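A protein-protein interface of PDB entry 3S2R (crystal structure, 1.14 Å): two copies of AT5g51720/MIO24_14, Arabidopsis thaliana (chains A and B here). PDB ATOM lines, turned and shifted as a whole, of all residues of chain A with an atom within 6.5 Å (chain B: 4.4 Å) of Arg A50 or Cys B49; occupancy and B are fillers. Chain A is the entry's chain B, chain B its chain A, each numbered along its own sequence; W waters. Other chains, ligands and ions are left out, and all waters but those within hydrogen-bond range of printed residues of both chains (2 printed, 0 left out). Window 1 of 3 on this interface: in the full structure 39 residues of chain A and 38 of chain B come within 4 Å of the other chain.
The indole nitrogen of Trp B52 lies within hydrogen-bond range of the backbone carbonyl oxygen of Arg A50 (2.8 Å). O of Arg B50 is in hydrogen-bond range of NE1 of Trp A52. NH2 of Arg A50 sits at hydrogen-bond distance from O of Val B32 (3.0 Å). N of Asp B34 is in hydrogen-bond range of O of Pro A77, 3.5 Å away. O of Val B32 lies close to N of Gly A76 (3.2 Å). OD2 of Asp B34 lies within salt-bridge range of NH1 of Arg A50 (2.8 Å). The backbone carbonyl oxygen of Asp B34 sits at hydrogen-bond distance from the backbone NH of Leu A79.
Of the printed residues of chain B, Arg A50 touches Val B32, Val B33, Asp B34, Cys B49, Arg B50, Trp B52, Phe B57 and Pro B58. Cys B49 touches just one residue of chain A: Arg A50 (3.5 Å). Of the printed residues of chain B, Cys A49 touches Arg B50. Of the printed residues of chain B, Gly A76 touches Val B32 (3.1 Å) and Trp B52 (3.7 Å). Of the printed residues of chain B, Pro A58 touches Arg B50 (3.8 Å). Of the printed residues of chain B, Leu A79 touches Val B33 and Asp B34. Of the printed residues of chain A, Cys B51 touches Ile A21 (3.7 Å). Cys A60 touches none of the printed residues of chain B. The nearest printed residue of chain B that does not touch Arg A50 is Cys B51 (5.5 Å). The nearest printed residue of chain B that does not touch Pro A58 is Cys B49 (10.0 Å).
Water W2 lies within hydrogen-bond range of the backbone carbonyl oxygen (O) of Cys A49 (2.7 Å), the backbone carbonyl oxygen (O) of Pro A58 (2.8 Å) and the guanidinium group (NH1) of Arg B50 (2.9 Å). Water W1 lies within hydrogen-bond range of the backbone carbonyl oxygen (O) of Cys B49 (2.7 Å), the guanidinium group (NH1) of Arg A50 (2.8 Å) and the backbone carbonyl oxygen (O) of Pro B58 (2.9 Å).
Arg B50 touches its own counterpart, Arg A50. Arg A50 touches Trp B52, and with the chains exchanged Trp A52 touches Arg B50. Arg A50 touches Phe B57, and with the chains exchanged Phe A57 touches Arg B50. Arg A50 touches Pro B58, and with the chains exchanged Pro A58 touches Arg B50. Positions printed for both chains: 48, 49, 50, 51, 52, 53, 57, 58 and 60. Of the 24 pairs that touch across the chains among the printed residues, 9 have their exchanged pair printed and touching as well.
Among the printed residues, pairs that only touch across the chains: Ile A21 with Arg B50 (3.8 Å), Ile A21 with Cys B51 (3.7 Å), Ile A21 with Arg B53 (3.8 Å), Cys A49 with Arg B50 (3.5 Å), Arg A50 with Val B33 (3.7 Å), Arg A50 with Cys B49 (3.5 Å), Arg A50 with Arg B50 (3.7 Å), Arg A50 with Phe B57 (3.4 Å), Arg A50 with Pro B58 (3.8 Å), Phe A57 with Arg B50 (3.4 Å), Pro A58 with Arg B50 (3.8 Å), Val A75 with Trp B52 (3.5 Å), Gly A76 with Trp B52 (3.7 Å), Pro A77 with Val B33 (3.4 Å), Leu A78 with Asp B34 (3.5 Å), Leu A78 with Tyr B48 (3.7 Å) and Leu A79 with Val B33 (3.7 Å).
Hydrophobic or aromatic side chains of chain B within 4 Å of the printed part of chain A: Val B33, Tyr B48, Trp B52, Phe B57 and Pro B58. Printed residues of chain A that touch a printed residue of chain B: Ile A21, Cys A49, Arg A50, Trp A52, Phe A57, Pro A58, Val A75, Gly A76, Pro A77, Leu A78 and Leu A79. Hydrophobic or aromatic side chains of chain A within 4 Å of the printed part of chain B: Ile A21, Trp A52, Phe A57, Pro A58, Val A75, Pro A77, Leu A78 and Leu A79. Among the printed residues, 24 pairs touch across the chains. Among the printed residues, Asp or Glu carboxylates within 4 Å of a Lys or Arg side-chain nitrogen of the other chain: Arg A50 with Asp B34.
The side-chain sulfur of Cys A49 lies close to the backbone NH of Trp A52, at 3.4 Å. The side-chain hydroxyl (OG) of Ser B54 lies within hydrogen-bond range of the backbone NH (N) of Phe B57, 3.4 Å away. The side-chain sulfur (SG) of Cys B49 lies close to the backbone NH (N) of Trp B52, at 3.3 Å. O of Gly A76 sits at hydrogen-bond distance from NE of Arg A50 (2.9 Å). The backbone carbonyl oxygen (O) of Pro B58 lies within hydrogen-bond range of the backbone NH (N) of Cys B49. The backbone NH (N) of Cys A49 lies within hydrogen-bond range of the backbone carbonyl oxygen (O) of Pro A58 (2.8 Å).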
ATOM      1  N   ILE A  21      42.248  26.228 -14.301  1.00  0.00           N
ATOM      2  CA  ILE A  21      41.245  25.298 -14.827  1.00  0.00           C
ATOM      3  C   ILE A  21      40.842  25.583 -16.276  1.00  0.00           C
ATOM      4  O   ILE A  21      40.108  24.772 -16.872  1.00  0.00           O
ATOM      5  CB  ILE A  21      39.981  25.264 -13.991  1.00  0.00           C
ATOM      6  CG1 ILE A  21      39.262  26.614 -14.010  1.00  0.00           C
ATOM      7  CG2 ILE A  21      40.275  24.829 -12.577  1.00  0.00           C
ATOM      8  CD1 ILE A  21      37.816  26.601 -13.388  1.00  0.00           C
ATOM      9  N   TYR A  48      24.598  25.275 -20.233  1.00  0.00           N
ATOM     10  CA  TYR A  48      25.748  26.145 -20.239  1.00  0.00           C
ATOM     11  C   TYR A  48      26.932  25.437 -19.591  1.00  0.00           C
ATOM     12  O   TYR A  48      26.822  24.786 -18.561  1.00  0.00           O
ATOM     13  CB  TYR A  48      25.437  27.479 -19.562  1.00  0.00           C
ATOM     14  CG  TYR A  48      24.776  28.435 -20.500  1.00  0.00           C
ATOM     15  CD1 TYR A  48      25.486  29.492 -21.079  1.00  0.00           C
ATOM     16  CD2 TYR A  48      23.455  28.269 -20.890  1.00  0.00           C
ATOM     17  CE1 TYR A  48      24.883  30.343 -22.013  1.00  0.00           C
ATOM     18  CE2 TYR A  48      22.857  29.135 -21.798  1.00  0.00           C
ATOM     19  CZ  TYR A  48      23.584  30.158 -22.367  1.00  0.00           C
ATOM     20  OH  TYR A  48      23.021  30.999 -23.304  1.00  0.00           O
ATOM     21  N   CYS A  49      28.097  25.614 -20.199  1.00  0.00           N
ATOM     22  CA  CYS A  49      29.319  24.956 -19.803  1.00  0.00           C
ATOM     23  C   CYS A  49      29.915  25.491 -18.520  1.00  0.00           C
ATOM     24  O   CYS A  49      30.060  26.706 -18.314  1.00  0.00           O
ATOM     25  CB  CYS A  49      30.354  25.097 -20.960  1.00  0.00           C
ATOM     26  SG  CYS A  49      31.918  24.204 -20.652  1.00  0.00           S
ATOM     27  N   ARG A  50      30.291  24.561 -17.656  1.00  0.00           N
ATOM     28  CA  ARG A  50      31.052  24.881 -16.437  1.00  0.00           C
ATOM     29  C   ARG A  50      32.397  24.169 -16.398  1.00  0.00           C
ATOM     30  O   ARG A  50      33.041  24.137 -15.354  1.00  0.00           O
ATOM     31  CB  ARG A  50      30.222  24.562 -15.208  1.00  0.00           C
ATOM     32  CG  ARG A  50      28.886  25.363 -15.183  1.00  0.00           C
ATOM     33  CD  ARG A  50      28.167  25.263 -13.862  1.00  0.00           C
ATOM     34  NE  ARG A  50      27.688  23.894 -13.610  1.00  0.00           N
ATOM     35  CZ  ARG A  50      26.926  23.560 -12.581  1.00  0.00           C
ATOM     36  NH1 ARG A  50      26.452  24.483 -11.749  1.00  0.00           N
ATOM     37  NH2 ARG A  50      26.592  22.284 -12.390  1.00  0.00           N
ATOM     38  N   CYS A  51      32.833  23.631 -17.545  1.00  0.00           N
ATOM     39  CA  CYS A  51      34.066  22.858 -17.573  1.00  0.00           C
ATOM     40  C   CYS A  51      35.169  23.487 -18.372  1.00  0.00           C
ATOM     41  O   CYS A  51      36.297  22.998 -18.312  1.00  0.00           O
ATOM     42  CB  CYS A  51      33.817  21.421 -18.063  1.00  0.00           C
ATOM     43  SG  CYS A  51      33.586  21.225 -19.830  1.00  0.00           S
ATOM     44  N   TRP A  52      34.898  24.560 -19.108  1.00  0.00           N
ATOM     45  CA  TRP A  52      35.944  25.241 -19.864  1.00  0.00           C
ATOM     46  C   TRP A  52      36.570  24.342 -20.915  1.00  0.00           C
ATOM     47  O   TRP A  52      37.744  24.527 -21.263  1.00  0.00           O
ATOM     48  CB  TRP A  52      37.002  25.862 -18.942  1.00  0.00           C
ATOM     49  CG  TRP A  52      36.323  26.829 -18.008  1.00  0.00           C
ATOM     50  CD1 TRP A  52      35.747  26.510 -16.832  1.00  0.00           C
ATOM     51  CD2 TRP A  52      36.106  28.239 -18.219  1.00  0.00           C
ATOM     52  NE1 TRP A  52      35.175  27.646 -16.263  1.00  0.00           N
ATOM     53  CE2 TRP A  52      35.362  28.705 -17.102  1.00  0.00           C
ATOM     54  CE3 TRP A  52      36.467  29.160 -19.217  1.00  0.00           C
ATOM     55  CZ2 TRP A  52      35.000  30.045 -16.966  1.00  0.00           C
ATOM     56  CZ3 TRP A  52      36.094  30.497 -19.068  1.00  0.00           C
ATOM     57  CH2 TRP A  52      35.351  30.919 -17.956  1.00  0.00           C
ATOM     58  N   ARG A  53      35.808  23.386 -21.432  1.00  0.00           N
ATOM     59  CA  ARG A  53      36.311  22.494 -22.512  1.00  0.00           C
ATOM     60  C   ARG A  53      35.406  22.497 -23.729  1.00  0.00           C
ATOM     61  O   ARG A  53      35.764  21.954 -24.765  1.00  0.00           O
ATOM     62  CB  ARG A  53      36.516  21.048 -22.024  1.00  0.00           C
ATOM     63  CG  ARG A  53      37.459  20.850 -20.835  1.00  0.00           C
ATOM     64  CD  ARG A  53      38.903  21.289 -21.125  1.00  0.00           C
ATOM     65  NE  ARG A  53      39.785  21.054 -19.987  1.00  0.00           N
ATOM     66  CZ  ARG A  53      40.030  21.967 -19.054  1.00  0.00           C
ATOM     67  NH1 ARG A  53      39.438  23.168 -19.138  1.00  0.00           N
ATOM     68  NH2 ARG A  53      40.842  21.681 -18.036  1.00  0.00           N
ATOM     69  N   PHE A  57      31.637  26.825 -26.197  1.00  0.00           N
ATOM     70  CA  PHE A  57      31.633  27.628 -24.982  1.00  0.00           C
ATOM     71  C   PHE A  57      31.100  29.039 -25.323  1.00  0.00           C
ATOM     72  O   PHE A  57      31.531  29.633 -26.307  1.00  0.00           O
ATOM     73  CB  PHE A  57      33.049  27.711 -24.408  1.00  0.00           C
ATOM     74  CG  PHE A  57      33.086  28.288 -23.030  1.00  0.00           C
ATOM     75  CD1 PHE A  57      33.227  29.668 -22.829  1.00  0.00           C
ATOM     76  CD2 PHE A  57      33.009  27.443 -21.927  1.00  0.00           C
ATOM     77  CE1 PHE A  57      33.232  30.203 -21.558  1.00  0.00           C
ATOM     78  CE2 PHE A  57      32.980  27.973 -20.640  1.00  0.00           C
ATOM     79  CZ  PHE A  57      33.115  29.339 -20.440  1.00  0.00           C
ATOM     80  N   PRO A  58      30.170  29.600 -24.518  1.00  0.00           N
ATOM     81  CA  PRO A  58      29.734  29.204 -23.182  1.00  0.00           C
ATOM     82  C   PRO A  58      28.688  28.092 -23.087  1.00  0.00           C
ATOM     83  O   PRO A  58      28.264  27.777 -21.991  1.00  0.00           O
ATOM     84  CB  PRO A  58      29.201  30.525 -22.599  1.00  0.00           C
ATOM     85  CG  PRO A  58      28.648  31.235 -23.766  1.00  0.00           C
ATOM     86  CD  PRO A  58      29.661  30.945 -24.860  1.00  0.00           C
ATOM     87  N   CYS A  60      27.310  24.127 -23.351  1.00  0.00           N
ATOM     88  CA  CYS A  60      27.812  22.766 -23.139  1.00  0.00           C
ATOM     89  C   CYS A  60      27.646  21.930 -24.389  1.00  0.00           C
ATOM     90  O   CYS A  60      26.546  21.865 -24.936  1.00  0.00           O
ATOM     91  CB  CYS A  60      27.002  22.155 -21.990  1.00  0.00           C
ATOM     92  SG  CYS A  60      27.304  20.393 -21.701  1.00  0.00           S
ATOM     93  N   VAL A  75      32.335  17.185 -13.176  1.00  0.00           N
ATOM     94  CA  VAL A  75      31.726  18.470 -13.511  1.00  0.00           C
ATOM     95  C   VAL A  75      30.624  18.269 -14.542  1.00  0.00           C
ATOM     96  O   VAL A  75      30.538  17.246 -15.214  1.00  0.00           O
ATOM     97  CB  VAL A  75      32.737  19.525 -14.013  1.00  0.00           C
ATOM     98  CG1 VAL A  75      33.732  19.868 -12.898  1.00  0.00           C
ATOM     99  CG2 VAL A  75      33.449  19.037 -15.245  1.00  0.00           C
ATOM    100  N   GLY A  76      29.726  19.229 -14.617  1.00  0.00           N
ATOM    101  CA  GLY A  76      28.643  19.193 -15.567  1.00  0.00           C
ATOM    102  C   GLY A  76      28.006  20.549 -15.718  1.00  0.00           C
ATOM    103  O   GLY A  76      28.380  21.495 -15.018  1.00  0.00           O
ATOM    104  N   PRO A  77      27.039  20.666 -16.624  1.00  0.00           N
ATOM    105  CA  PRO A  77      26.557  21.969 -17.025  1.00  0.00           C
ATOM    106  C   PRO A  77      25.469  22.547 -16.097  1.00  0.00           C
ATOM    107  O   PRO A  77      24.916  21.868 -15.207  1.00  0.00           O
ATOM    108  CB  PRO A  77      25.895  21.680 -18.396  1.00  0.00           C
ATOM    109  CG  PRO A  77      25.482  20.244 -18.321  1.00  0.00           C
ATOM    110  CD  PRO A  77      26.610  19.617 -17.589  1.00  0.00           C
ATOM    111  N   LEU A  78      25.215  23.815 -16.306  1.00  0.00           N
ATOM    112  CA  LEU A  78      24.080  24.563 -15.716  1.00  0.00           C
ATOM    113  C   LEU A  78      22.941  24.587 -16.717  1.00  0.00           C
ATOM    114  O   LEU A  78      23.133  25.001 -17.856  1.00  0.00           O
ATOM    115  CB  LEU A  78      24.564  25.967 -15.381  1.00  0.00           C
ATOM    116  CG  LEU A  78      23.505  26.837 -14.684  1.00  0.00           C
ATOM    117  CD1 LEU A  78      23.276  26.353 -13.240  1.00  0.00           C
ATOM    118  CD2 LEU A  78      24.002  28.291 -14.647  1.00  0.00           C
ATOM    119  N   LEU A  79      21.751  24.135 -16.315  1.00  0.00           N
ATOM    120  CA  LEU A  79      20.619  24.047 -17.216  1.00  0.00           C
ATOM    121  C   LEU A  79      19.733  25.250 -17.017  1.00  0.00           C
ATOM    122  O   LEU A  79      19.154  25.403 -15.942  1.00  0.00           O
ATOM    123  CB  LEU A  79      19.776  22.766 -16.964  1.00  0.00           C
ATOM    124  CG  LEU A  79      20.583  21.467 -16.986  1.00  0.00           C
ATOM    125  CD1 LEU A  79      19.646  20.272 -16.824  1.00  0.00           C
ATOM    126  CD2 LEU A  79      21.395  21.298 -18.286  1.00  0.00           C
ATOM    127  N   VAL B  32      27.860  16.671 -11.815  1.00  0.00           N
ATOM    128  CA  VAL B  32      27.134  17.708 -11.064  1.00  0.00           C
ATOM    129  C   VAL B  32      26.468  18.660 -12.057  1.00  0.00           C
ATOM    130  O   VAL B  32      27.125  19.355 -12.814  1.00  0.00           O
ATOM    131  CB  VAL B  32      28.098  18.488 -10.124  1.00  0.00           C
ATOM    132  CG1 VAL B  32      27.411  19.644  -9.466  1.00  0.00           C
ATOM    133  CG2 VAL B  32      28.727  17.527  -9.097  1.00  0.00           C
ATOM    134  N   VAL B  33      25.141  18.644 -12.025  1.00  0.00           N
ATOM    135  CA  VAL B  33      24.308  19.466 -12.843  1.00  0.00           C
ATOM    136  C   VAL B  33      23.389  20.274 -11.927  1.00  0.00           C
ATOM    137  O   VAL B  33      23.024  19.822 -10.832  1.00  0.00           O
ATOM    138  CB  VAL B  33      23.517  18.624 -13.828  1.00  0.00           C
ATOM    139  CG1 VAL B  33      22.599  19.423 -14.613  1.00  0.00           C
ATOM    140  CG2 VAL B  33      24.435  17.978 -14.839  1.00  0.00           C
ATOM    141  N   ASP B  34      23.097  21.511 -12.290  1.00  0.00           N
ATOM    142  CA  ASP B  34      22.154  22.371 -11.555  1.00  0.00           C
ATOM    143  C   ASP B  34      21.237  22.978 -12.549  1.00  0.00           C
ATOM    144  O   ASP B  34      21.626  23.216 -13.695  1.00  0.00           O
ATOM    145  CB  ASP B  34      22.891  23.444 -10.779  1.00  0.00           C
ATOM    146  CG  ASP B  34      23.808  22.840  -9.721  1.00  0.00           C
ATOM    147  OD1 ASP B  34      23.250  22.466  -8.665  1.00  0.00           O
ATOM    148  OD2 ASP B  34      25.055  22.816  -9.909  1.00  0.00           O
ATOM    149  N   PRO B  47      24.893  35.945 -10.570  1.00  0.00           N
ATOM    150  CA  PRO B  47      26.092  35.278 -11.088  1.00  0.00           C
ATOM    151  C   PRO B  47      26.151  33.806 -10.658  1.00  0.00           C
ATOM    152  O   PRO B  47      26.009  33.495  -9.468  1.00  0.00           O
ATOM    153  CB  PRO B  47      27.209  36.098 -10.442  1.00  0.00           C
ATOM    154  CG  PRO B  47      26.640  36.463  -9.050  1.00  0.00           C
ATOM    155  CD  PRO B  47      25.168  36.683  -9.301  1.00  0.00           C
ATOM    156  N   TYR B  48      26.361  32.930 -11.653  1.00  0.00           N
ATOM    157  CA  TYR B  48      26.481  31.515 -11.440  1.00  0.00           C
ATOM    158  C   TYR B  48      27.952  31.053 -11.609  1.00  0.00           C
ATOM    159  O   TYR B  48      28.608  31.459 -12.565  1.00  0.00           O
ATOM    160  CB  TYR B  48      25.541  30.737 -12.368  1.00  0.00           C
ATOM    161  CG  TYR B  48      24.172  30.641 -11.745  1.00  0.00           C
ATOM    162  CD1 TYR B  48      23.781  29.490 -11.057  1.00  0.00           C
ATOM    163  CD2 TYR B  48      23.291  31.726 -11.745  1.00  0.00           C
ATOM    164  CE1 TYR B  48      22.530  29.426 -10.399  1.00  0.00           C
ATOM    165  CE2 TYR B  48      22.053  31.660 -11.108  1.00  0.00           C
ATOM    166  CZ  TYR B  48      21.691  30.516 -10.430  1.00  0.00           C
ATOM    167  OH  TYR B  48      20.480  30.459  -9.785  1.00  0.00           O
ATOM    168  N   CYS B  49      28.433  30.239 -10.694  1.00  0.00           N
ATOM    169  CA  CYS B  49      29.823  29.856 -10.642  1.00  0.00           C
ATOM    170  C   CYS B  49      30.196  28.923 -11.780  1.00  0.00           C
ATOM    171  O   CYS B  49      29.531  27.905 -12.049  1.00  0.00           O
ATOM    172  CB  CYS B  49      30.081  29.152  -9.314  1.00  0.00           C
ATOM    173  SG  CYS B  49      31.802  28.696  -9.001  1.00  0.00           S
ATOM    174  N   ARG B  50      31.348  29.217 -12.382  1.00  0.00           N
ATOM    175  CA  ARG B  50      31.970  28.342 -13.403  1.00  0.00           C
ATOM    176  C   ARG B  50      33.368  27.913 -12.946  1.00  0.00           C
ATOM    177  O   ARG B  50      34.079  27.304 -13.735  1.00  0.00           O
ATOM    178  CB  ARG B  50      32.019  28.985 -14.779  1.00  0.00           C
ATOM    179  CG  ARG B  50      30.604  29.323 -15.267  1.00  0.00           C
ATOM    180  CD  ARG B  50      30.583  29.735 -16.719  1.00  0.00           C
ATOM    181  NE  ARG B  50      31.279  31.012 -16.934  1.00  0.00           N
ATOM    182  CZ  ARG B  50      31.318  31.660 -18.095  1.00  0.00           C
ATOM    183  NH1 ARG B  50      30.593  31.212 -19.107  1.00  0.00           N
ATOM    184  NH2 ARG B  50      32.035  32.752 -18.230  1.00  0.00           N
ATOM    185  N   CYS B  51      33.734  28.197 -11.690  1.00  0.00           N
ATOM    186  CA  CYS B  51      35.077  27.908 -11.226  1.00  0.00           C
ATOM    187  C   CYS B  51      35.154  26.770 -10.202  1.00  0.00           C
ATOM    188  O   CYS B  51      36.244  26.325  -9.849  1.00  0.00           O
ATOM    189  CB  CYS B  51      35.764  29.193 -10.691  1.00  0.00           C
ATOM    190  SG  CYS B  51      35.242  29.677  -9.038  1.00  0.00           S
ATOM    191  N   TRP B  52      34.010  26.346  -9.679  1.00  0.00           N
ATOM    192  CA  TRP B  52      33.900  25.239  -8.727  1.00  0.00           C
ATOM    193  C   TRP B  52      34.584  25.530  -7.379  1.00  0.00           C
ATOM    194  O   TRP B  52      34.921  24.580  -6.656  1.00  0.00           O
ATOM    195  CB  TRP B  52      34.419  23.916  -9.349  1.00  0.00           C
ATOM    196  CG  TRP B  52      33.624  23.601 -10.559  1.00  0.00           C
ATOM    197  CD1 TRP B  52      33.839  24.084 -11.811  1.00  0.00           C
ATOM    198  CD2 TRP B  52      32.450  22.767 -10.624  1.00  0.00           C
ATOM    199  NE1 TRP B  52      32.853  23.615 -12.653  1.00  0.00           N
ATOM    200  CE2 TRP B  52      31.995  22.806 -11.953  1.00  0.00           C
ATOM    201  CE3 TRP B  52      31.742  21.995  -9.698  1.00  0.00           C
ATOM    202  CZ2 TRP B  52      30.836  22.111 -12.364  1.00  0.00           C
ATOM    203  CZ3 TRP B  52      30.643  21.261 -10.122  1.00  0.00           C
ATOM    204  CH2 TRP B  52      30.198  21.338 -11.440  1.00  0.00           C
ATOM    205  N   ARG B  53      34.778  26.816  -7.061  1.00  0.00           N
ATOM    206  CA  ARG B  53      35.413  27.244  -5.805  1.00  0.00           C
ATOM    207  C   ARG B  53      34.446  27.994  -4.889  1.00  0.00           C
ATOM    208  O   ARG B  53      34.805  28.283  -3.755  1.00  0.00           O
ATOM    209  CB  ARG B  53      36.661  28.132  -6.042  1.00  0.00           C
ATOM    210  CG  ARG B  53      37.752  27.648  -7.003  1.00  0.00           C
ATOM    211  CD  ARG B  53      38.141  26.297  -6.599  1.00  0.00           C
ATOM    212  NE  ARG B  53      39.431  25.793  -7.121  1.00  0.00           N
ATOM    213  CZ  ARG B  53      39.601  25.133  -8.275  1.00  0.00           C
ATOM    214  NH1 ARG B  53      38.592  24.957  -9.129  1.00  0.00           N
ATOM    215  NH2 ARG B  53      40.786  24.605  -8.562  1.00  0.00           N
ATOM    216  N   SER B  54      33.279  28.356  -5.394  1.00  0.00           N
ATOM    217  CA  SER B  54      32.328  29.151  -4.621  1.00  0.00           C
ATOM    218  C   SER B  54      31.828  28.449  -3.380  1.00  0.00           C
ATOM    219  O   SER B  54      31.427  27.271  -3.437  1.00  0.00           O
ATOM    220  CB  SER B  54      31.110  29.565  -5.433  1.00  0.00           C
ATOM    221  OG  SER B  54      30.243  30.267  -4.577  1.00  0.00           O
ATOM    222  N   PHE B  57      28.158  27.642  -4.213  1.00  0.00           N
ATOM    223  CA  PHE B  57      27.938  26.913  -5.440  1.00  0.00           C
ATOM    224  C   PHE B  57      26.532  26.300  -5.456  1.00  0.00           C
ATOM    225  O   PHE B  57      26.116  25.692  -4.477  1.00  0.00           O
ATOM    226  CB  PHE B  57      28.996  25.829  -5.598  1.00  0.00           C
ATOM    227  CG  PHE B  57      29.028  25.246  -6.969  1.00  0.00           C
ATOM    228  CD1 PHE B  57      29.846  25.798  -7.906  1.00  0.00           C
ATOM    229  CD2 PHE B  57      28.205  24.146  -7.293  1.00  0.00           C
ATOM    230  CE1 PHE B  57      29.835  25.342  -9.215  1.00  0.00           C
ATOM    231  CE2 PHE B  57      28.192  23.666  -8.657  1.00  0.00           C
ATOM    232  CZ  PHE B  57      29.041  24.249  -9.569  1.00  0.00           C
ATOM    233  N   PRO B  58      25.733  26.478  -6.517  1.00  0.00           N
ATOM    234  CA  PRO B  58      26.105  26.922  -7.855  1.00  0.00           C
ATOM    235  C   PRO B  58      26.165  28.439  -8.069  1.00  0.00           C
ATOM    236  O   PRO B  58      26.505  28.834  -9.175  1.00  0.00           O
ATOM    237  CB  PRO B  58      25.015  26.280  -8.725  1.00  0.00           C
ATOM    238  CG  PRO B  58      23.767  26.283  -7.812  1.00  0.00           C
ATOM    239  CD  PRO B  58      24.373  25.880  -6.473  1.00  0.00           C
ATOM    240  N   LEU B  59      25.877  29.240  -7.058  1.00  0.00           N
ATOM    241  CA  LEU B  59      26.070  30.686  -7.193  1.00  0.00           C
ATOM    242  C   LEU B  59      27.557  31.035  -7.124  1.00  0.00           C
ATOM    243  O   LEU B  59      28.337  30.331  -6.485  1.00  0.00           O
ATOM    244  CB  LEU B  59      25.281  31.480  -6.144  1.00  0.00           C
ATOM    245  CG  LEU B  59      23.758  31.355  -6.232  1.00  0.00           C
ATOM    246  CD1 LEU B  59      23.106  31.930  -4.980  1.00  0.00           C
ATOM    247  CD2 LEU B  59      23.237  32.088  -7.467  1.00  0.00           C
ATOM    248  N   CYS B  60      27.926  32.158  -7.744  1.00  0.00           N
ATOM    249  CA  CYS B  60      29.269  32.758  -7.664  1.00  0.00           C
ATOM    250  C   CYS B  60      29.375  33.654  -6.421  1.00  0.00           C
ATOM    251  O   CYS B  60      28.467  34.488  -6.240  1.00  0.00           O
ATOM    252  CB  CYS B  60      29.508  33.531  -8.961  1.00  0.00           C
ATOM    253  SG  CYS B  60      30.962  34.673  -8.904  1.00  0.00           S
HETATM  254  O   HOH W   1      26.916  27.275 -11.547  1.00  0.00           O
HETATM  255  O   HOH W   2      28.952  28.894 -19.478  1.00  0.00           O
